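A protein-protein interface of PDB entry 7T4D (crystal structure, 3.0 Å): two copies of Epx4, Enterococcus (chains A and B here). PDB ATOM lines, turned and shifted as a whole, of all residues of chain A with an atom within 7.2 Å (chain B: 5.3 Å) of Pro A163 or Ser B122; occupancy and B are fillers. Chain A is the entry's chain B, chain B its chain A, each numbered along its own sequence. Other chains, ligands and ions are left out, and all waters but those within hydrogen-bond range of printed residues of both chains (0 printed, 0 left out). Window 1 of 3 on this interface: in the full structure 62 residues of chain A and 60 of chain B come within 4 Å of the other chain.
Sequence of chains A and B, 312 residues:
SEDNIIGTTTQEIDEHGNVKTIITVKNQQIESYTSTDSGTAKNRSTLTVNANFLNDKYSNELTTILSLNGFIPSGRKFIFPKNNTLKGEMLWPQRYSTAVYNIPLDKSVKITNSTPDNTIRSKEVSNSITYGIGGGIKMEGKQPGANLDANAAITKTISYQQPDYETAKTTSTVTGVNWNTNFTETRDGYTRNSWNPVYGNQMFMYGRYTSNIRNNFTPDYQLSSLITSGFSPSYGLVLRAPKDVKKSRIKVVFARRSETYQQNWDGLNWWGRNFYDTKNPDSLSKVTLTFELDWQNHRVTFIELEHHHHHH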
ATOM      1  N   ARG A 121     -25.770  15.016  20.058  1.00  0.00           N
ATOM      2  CA  ARG A 121     -26.619  15.949  19.332  1.00  0.00           C
ATOM      3  C   ARG A 121     -28.100  15.686  19.600  1.00  0.00           C
ATOM      4  O   ARG A 121     -28.462  14.660  20.177  1.00  0.00           O
ATOM      5  CB  ARG A 121     -26.314  15.863  17.837  1.00  0.00           C
ATOM      6  CG  ARG A 121     -24.938  16.404  17.470  1.00  0.00           C
ATOM      7  CD  ARG A 121     -24.674  16.302  15.977  1.00  0.00           C
ATOM      8  NE  ARG A 121     -25.857  16.604  15.177  1.00  0.00           N
ATOM      9  CZ  ARG A 121     -26.068  17.760  14.557  1.00  0.00           C
ATOM     10  NH1 ARG A 121     -25.171  18.734  14.639  1.00  0.00           N
ATOM     11  NH2 ARG A 121     -27.177  17.939  13.852  1.00  0.00           N
ATOM     12  N   TYR A 160     -33.607  19.001  12.374  1.00  0.00           N
ATOM     13  CA  TYR A 160     -32.243  19.008  12.891  1.00  0.00           C
ATOM     14  C   TYR A 160     -31.303  19.896  12.072  1.00  0.00           C
ATOM     15  O   TYR A 160     -31.696  20.479  11.061  1.00  0.00           O
ATOM     16  CB  TYR A 160     -31.695  17.579  12.946  1.00  0.00           C
ATOM     17  CG  TYR A 160     -31.765  16.833  11.631  1.00  0.00           C
ATOM     18  CD1 TYR A 160     -30.733  16.914  10.704  1.00  0.00           C
ATOM     19  CD2 TYR A 160     -32.864  16.044  11.318  1.00  0.00           C
ATOM     20  CE1 TYR A 160     -30.797  16.231   9.501  1.00  0.00           C
ATOM     21  CE2 TYR A 160     -32.937  15.359  10.120  1.00  0.00           C
ATOM     22  CZ  TYR A 160     -31.902  15.455   9.215  1.00  0.00           C
ATOM     23  OH  TYR A 160     -31.975  14.772   8.022  1.00  0.00           O
ATOM     24  N   GLN A 161     -30.055  19.986  12.523  1.00  0.00           N
ATOM     25  CA  GLN A 161     -29.031  20.766  11.841  1.00  0.00           C
ATOM     26  C   GLN A 161     -28.012  19.825  11.212  1.00  0.00           C
ATOM     27  O   GLN A 161     -27.571  18.868  11.846  1.00  0.00           O
ATOM     28  CB  GLN A 161     -28.340  21.722  12.813  1.00  0.00           C
ATOM     29  CG  GLN A 161     -29.224  22.847  13.324  1.00  0.00           C
ATOM     30  CD  GLN A 161     -29.017  24.139  12.558  1.00  0.00           C
ATOM     31  OE1 GLN A 161     -27.886  24.514  12.248  1.00  0.00           O
ATOM     32  NE2 GLN A 161     -30.112  24.824  12.244  1.00  0.00           N
ATOM     33  N   GLN A 162     -27.643  20.088   9.964  1.00  0.00           N
ATOM     34  CA  GLN A 162     -26.765  19.178   9.241  1.00  0.00           C
ATOM     35  C   GLN A 162     -25.551  19.889   8.657  1.00  0.00           C
ATOM     36  O   GLN A 162     -25.677  20.650   7.699  1.00  0.00           O
ATOM     37  CB  GLN A 162     -27.539  18.473   8.129  1.00  0.00           C
ATOM     38  CG  GLN A 162     -26.694  17.527   7.305  1.00  0.00           C
ATOM     39  CD  GLN A 162     -26.509  16.190   7.988  1.00  0.00           C
ATOM     40  OE1 GLN A 162     -27.423  15.366   8.018  1.00  0.00           O
ATOM     41  NE2 GLN A 162     -25.326  15.973   8.555  1.00  0.00           N
ATOM     42  N   PRO A 163     -24.366  19.642   9.237  1.00  0.00           N
ATOM     43  CA  PRO A 163     -23.128  20.214   8.698  1.00  0.00           C
ATOM     44  C   PRO A 163     -22.715  19.516   7.406  1.00  0.00           C
ATOM     45  O   PRO A 163     -23.053  18.350   7.205  1.00  0.00           O
ATOM     46  CB  PRO A 163     -22.108  19.961   9.811  1.00  0.00           C
ATOM     47  CG  PRO A 163     -22.643  18.778  10.543  1.00  0.00           C
ATOM     48  CD  PRO A 163     -24.134  18.921  10.501  1.00  0.00           C
ATOM     49  N   ASP A 164     -21.995  20.225   6.546  1.00  0.00           N
ATOM     50  CA  ASP A 164     -21.532  19.658   5.286  1.00  0.00           C
ATOM     51  C   ASP A 164     -20.498  18.571   5.549  1.00  0.00           C
ATOM     52  O   ASP A 164     -20.369  17.618   4.779  1.00  0.00           O
ATOM     53  CB  ASP A 164     -20.950  20.750   4.390  1.00  0.00           C
ATOM     54  CG  ASP A 164     -21.977  21.801   4.011  1.00  0.00           C
ATOM     55  OD1 ASP A 164     -23.184  21.566   4.249  1.00  0.00           O
ATOM     56  OD2 ASP A 164     -21.583  22.864   3.481  1.00  0.00           O
ATOM     57  N   TYR A 165     -19.767  18.725   6.649  1.00  0.00           N
ATOM     58  CA  TYR A 165     -18.805  17.726   7.096  1.00  0.00           C
ATOM     59  C   TYR A 165     -18.960  17.475   8.593  1.00  0.00           C
ATOM     60  O   TYR A 165     -19.250  18.395   9.359  1.00  0.00           O
ATOM     61  CB  TYR A 165     -17.374  18.169   6.778  1.00  0.00           C
ATOM     62  CG  TYR A 165     -16.888  17.788   5.396  1.00  0.00           C
ATOM     63  CD1 TYR A 165     -17.330  18.463   4.266  1.00  0.00           C
ATOM     64  CD2 TYR A 165     -15.975  16.755   5.225  1.00  0.00           C
ATOM     65  CE1 TYR A 165     -16.879  18.116   3.003  1.00  0.00           C
ATOM     66  CE2 TYR A 165     -15.520  16.402   3.969  1.00  0.00           C
ATOM     67  CZ  TYR A 165     -15.974  17.084   2.862  1.00  0.00           C
ATOM     68  OH  TYR A 165     -15.524  16.734   1.610  1.00  0.00           O
ATOM     69  N   GLU A 166     -18.776  16.224   9.004  1.00  0.00           N
ATOM     70  CA  GLU A 166     -18.891  15.848  10.408  1.00  0.00           C
ATOM     71  C   GLU A 166     -17.535  15.470  11.000  1.00  0.00           C
ATOM     72  O   GLU A 166     -16.791  14.681  10.415  1.00  0.00           O
ATOM     73  CB  GLU A 166     -19.872  14.688  10.569  1.00  0.00           C
ATOM     74  CG  GLU A 166     -20.077  14.233  12.004  1.00  0.00           C
ATOM     75  CD  GLU A 166     -21.053  13.076  12.108  1.00  0.00           C
ATOM     76  OE1 GLU A 166     -21.551  12.625  11.054  1.00  0.00           O
ATOM     77  OE2 GLU A 166     -21.314  12.613  13.241  1.00  0.00           O
ATOM     78  N   THR A 167     -17.219  16.036  12.162  1.00  0.00           N
ATOM     79  CA  THR A 167     -15.960  15.740  12.837  1.00  0.00           C
ATOM     80  C   THR A 167     -16.176  14.966  14.132  1.00  0.00           C
ATOM     81  O   THR A 167     -17.014  15.332  14.955  1.00  0.00           O
ATOM     82  CB  THR A 167     -15.171  17.026  13.152  1.00  0.00           C
ATOM     83  OG1 THR A 167     -14.949  17.765  11.943  1.00  0.00           O
ATOM     84  CG2 THR A 167     -13.831  16.681  13.778  1.00  0.00           C
ATOM     85  N   ASN A 182     -15.548  13.805   8.035  1.00  0.00           N
ATOM     86  CA  ASN A 182     -16.148  13.070   6.932  1.00  0.00           C
ATOM     87  C   ASN A 182     -17.200  13.870   6.181  1.00  0.00           C
ATOM     88  O   ASN A 182     -17.884  14.720   6.753  1.00  0.00           O
ATOM     89  CB  ASN A 182     -16.784  11.775   7.441  1.00  0.00           C
ATOM     90  CG  ASN A 182     -15.839  10.951   8.287  1.00  0.00           C
ATOM     91  OD1 ASN A 182     -14.747  10.594   7.848  1.00  0.00           O
ATOM     92  ND2 ASN A 182     -16.251  10.648   9.513  1.00  0.00           N
ATOM     93  N   PHE A 183     -17.317  13.589   4.890  1.00  0.00           N
ATOM     94  CA  PHE A 183     -18.386  14.144   4.078  1.00  0.00           C
ATOM     95  C   PHE A 183     -19.705  13.511   4.499  1.00  0.00           C
ATOM     96  O   PHE A 183     -19.766  12.311   4.769  1.00  0.00           O
ATOM     97  CB  PHE A 183     -18.115  13.898   2.594  1.00  0.00           C
ATOM     98  CG  PHE A 183     -19.305  14.138   1.710  1.00  0.00           C
ATOM     99  CD1 PHE A 183     -19.594  15.407   1.236  1.00  0.00           C
ATOM    100  CD2 PHE A 183     -20.133  13.088   1.349  1.00  0.00           C
ATOM    101  CE1 PHE A 183     -20.688  15.622   0.422  1.00  0.00           C
ATOM    102  CE2 PHE A 183     -21.228  13.298   0.540  1.00  0.00           C
ATOM    103  CZ  PHE A 183     -21.506  14.565   0.073  1.00  0.00           C
ATOM    104  N   THR A 184     -20.758  14.316   4.557  1.00  0.00           N
ATOM    105  CA  THR A 184     -22.067  13.818   4.962  1.00  0.00           C
ATOM    106  C   THR A 184     -22.955  13.600   3.742  1.00  0.00           C
ATOM    107  O   THR A 184     -23.011  12.503   3.184  1.00  0.00           O
ATOM    108  CB  THR A 184     -22.766  14.786   5.936  1.00  0.00           C
ATOM    109  OG1 THR A 184     -22.891  16.075   5.323  1.00  0.00           O
ATOM    110  CG2 THR A 184     -21.971  14.916   7.227  1.00  0.00           C
ATOM    111  N   GLU A 185     -23.645  14.658   3.336  1.00  0.00           N
ATOM    112  CA  GLU A 185     -24.499  14.614   2.161  1.00  0.00           C
ATOM    113  C   GLU A 185     -24.426  15.941   1.418  1.00  0.00           C
ATOM    114  O   GLU A 185     -23.982  16.948   1.971  1.00  0.00           O
ATOM    115  CB  GLU A 185     -25.942  14.302   2.554  1.00  0.00           C
ATOM    116  CG  GLU A 185     -26.685  15.473   3.177  1.00  0.00           C
ATOM    117  CD  GLU A 185     -28.073  15.096   3.658  1.00  0.00           C
ATOM    118  OE1 GLU A 185     -28.901  16.010   3.865  1.00  0.00           O
ATOM    119  OE2 GLU A 185     -28.337  13.888   3.829  1.00  0.00           O
ATOM    120  N   ILE B 120     -16.882  25.300   7.741  1.00  0.00           N
ATOM    121  CA  ILE B 120     -17.876  24.296   7.391  1.00  0.00           C
ATOM    122  C   ILE B 120     -19.259  24.867   7.657  1.00  0.00           C
ATOM    123  O   ILE B 120     -19.533  25.362   8.750  1.00  0.00           O
ATOM    124  CB  ILE B 120     -17.698  22.992   8.192  1.00  0.00           C
ATOM    125  CG1 ILE B 120     -16.307  22.401   7.959  1.00  0.00           C
ATOM    126  CG2 ILE B 120     -18.770  21.986   7.807  1.00  0.00           C
ATOM    127  CD1 ILE B 120     -16.066  21.098   8.698  1.00  0.00           C
ATOM    128  N   ARG B 121     -20.131  24.799   6.658  1.00  0.00           N
ATOM    129  CA  ARG B 121     -21.451  25.396   6.780  1.00  0.00           C
ATOM    130  C   ARG B 121     -22.492  24.342   7.126  1.00  0.00           C
ATOM    131  O   ARG B 121     -22.214  23.144   7.088  1.00  0.00           O
ATOM    132  CB  ARG B 121     -21.845  26.124   5.493  1.00  0.00           C
ATOM    133  CG  ARG B 121     -21.036  27.379   5.219  1.00  0.00           C
ATOM    134  CD  ARG B 121     -21.526  28.086   3.967  1.00  0.00           C
ATOM    135  NE  ARG B 121     -21.856  29.483   4.236  1.00  0.00           N
ATOM    136  CZ  ARG B 121     -23.040  29.901   4.672  1.00  0.00           C
ATOM    137  NH1 ARG B 121     -24.016  29.030   4.889  1.00  0.00           N
ATOM    138  NH2 ARG B 121     -23.249  31.193   4.892  1.00  0.00           N
ATOM    139  N   SER B 122     -23.694  24.797   7.459  1.00  0.00           N
ATOM    140  CA  SER B 122     -24.768  23.893   7.841  1.00  0.00           C
ATOM    141  C   SER B 122     -26.076  24.269   7.161  1.00  0.00           C
ATOM    142  O   SER B 122     -26.199  25.335   6.558  1.00  0.00           O
ATOM    143  CB  SER B 122     -24.951  23.893   9.360  1.00  0.00           C
ATOM    144  OG  SER B 122     -23.731  23.593  10.015  1.00  0.00           O
ATOM    145  N   LYS B 123     -27.051  23.375   7.261  1.00  0.00           N
ATOM    146  CA  LYS B 123     -28.382  23.621   6.731  1.00  0.00           C
ATOM    147  C   LYS B 123     -29.418  23.078   7.702  1.00  0.00           C
ATOM    148  O   LYS B 123     -29.105  22.238   8.546  1.00  0.00           O
ATOM    149  CB  LYS B 123     -28.544  22.971   5.358  1.00  0.00           C
ATOM    150  CG  LYS B 123     -28.267  21.474   5.360  1.00  0.00           C
ATOM    151  CD  LYS B 123     -28.517  20.849   3.999  1.00  0.00           C
ATOM    152  CE  LYS B 123     -27.884  19.469   3.910  1.00  0.00           C
ATOM    153  NZ  LYS B 123     -28.549  18.609   2.890  1.00  0.00           N
ATOM    154  N   GLU B 124     -30.650  23.556   7.583  1.00  0.00           N
ATOM    155  CA  GLU B 124     -31.724  23.081   8.443  1.00  0.00           C
ATOM    156  C   GLU B 124     -32.572  22.065   7.689  1.00  0.00           C
ATOM    157  O   GLU B 124     -33.018  22.324   6.572  1.00  0.00           O
ATOM    158  CB  GLU B 124     -32.583  24.250   8.924  1.00  0.00           C
ATOM    159  CG  GLU B 124     -33.713  23.851   9.853  1.00  0.00           C
ATOM    160  CD  GLU B 124     -34.598  25.026  10.223  1.00  0.00           C
ATOM    161  OE1 GLU B 124     -34.236  26.173   9.885  1.00  0.00           O
ATOM    162  OE2 GLU B 124     -35.659  24.802  10.846  1.00  0.00           O
ATOM    163  N   SER B 159     -33.228  24.122   4.393  1.00  0.00           N
ATOM    164  CA  SER B 159     -33.061  25.571   4.434  1.00  0.00           C
ATOM    165  C   SER B 159     -31.623  25.975   4.752  1.00  0.00           C
ATOM    166  O   SER B 159     -30.983  25.386   5.623  1.00  0.00           O
ATOM    167  CB  SER B 159     -34.011  26.184   5.462  1.00  0.00           C
ATOM    168  OG  SER B 159     -35.307  25.623   5.353  1.00  0.00           O
ATOM    169  N   TYR B 160     -31.124  26.980   4.037  1.00  0.00           N
ATOM    170  CA  TYR B 160     -29.761  27.464   4.231  1.00  0.00           C
ATOM    171  C   TYR B 160     -29.637  28.939   3.852  1.00  0.00           C
ATOM    172  O   TYR B 160     -30.598  29.550   3.386  1.00  0.00           O
ATOM    173  CB  TYR B 160     -28.775  26.626   3.414  1.00  0.00           C
ATOM    174  CG  TYR B 160     -29.101  26.557   1.939  1.00  0.00           C
ATOM    175  CD1 TYR B 160     -28.620  27.513   1.055  1.00  0.00           C
ATOM    176  CD2 TYR B 160     -29.896  25.539   1.432  1.00  0.00           C
ATOM    177  CE1 TYR B 160     -28.917  27.452  -0.293  1.00  0.00           C
ATOM    178  CE2 TYR B 160     -30.199  25.472   0.086  1.00  0.00           C
ATOM    179  CZ  TYR B 160     -29.708  26.429  -0.771  1.00  0.00           C
ATOM    180  OH  TYR B 160     -30.008  26.364  -2.112  1.00  0.00           O
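O of Lys B123 lies within hydrogen-bond range of N of Gln A162. The backbone NH (N) of Asp A164 lies within hydrogen-bond range of the backbone carbonyl oxygen (O) of Arg B121, 3.0 Å away. The side-chain amino group (NZ) of Lys B123 is in salt-bridge range of the side-chain carboxylate (OE1) of Glu A185 (2.8 Å).
The backbone carbonyl oxygen (O) of Asp A164 sits at hydrogen-bond distance from the side-chain hydroxyl (OG1) of Thr A184, at 3.0 Å. N of Glu B124 is in hydrogen-bond range of O of Ser B159, 2.7 Å away. The backbone carbonyl oxygen (O) of Pro A163 is in hydrogen-bond range of the side-chain hydroxyl (OG1) of Thr A184, 3.0 Å away.
CA of Glu B124 touches O of Tyr A160, 3.7 Å away. CA of Gln A161 touches O of Lys B123 (3.6 Å). CA of Ser B122 touches O of Gln A162, at 3.4 Å. Arg B121 touches Pro A163 (O to CA, 3.5 Å). Pro A163 touches Ser B122 (CA to OG, 3.7 Å). Ile B120 touches Asp A164 (CG2 to N, 3.9 Å). Tyr A165 touches Ile B120.
Of the printed residues of chain B, Gln A161 touches Lys B123 (3.6 Å). Printed residues of chain B within 4 Å of Gln A162: Ser B122 and Lys B123. Of chain B, only Arg B121 and Ser B122 come within 4 Å of Pro A163. Of the printed residues of chain B, Glu A185 touches Lys B123. Of the printed residues of chain A, Ile B120 touches Asp A164 and Tyr A165. Of the printed residues of chain A, Arg B121 touches Pro A163 and Asp A164. Ser B122 touches just these residues of chain A: Gln A162 (3.4 Å) and Pro A163 (3.7 Å). The nearest residue of chain B that does not touch Pro A163 is Ile B120 (4.4 Å). The nearest residue of chain A that does not touch Ser B122 is Gln A161 (4.2 Å).
Along chain A the printed residues that touch a printed residue of chain B span positions 160 to 185. Among the printed residues, 10 pairs touch across the chains. Among the printed residues, Asp or Glu carboxylates within 4 Å of a Lys or Arg side-chain nitrogen of the other chain: Glu A185 with Lys B123.
Positions printed for both chains: 121 and 160.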
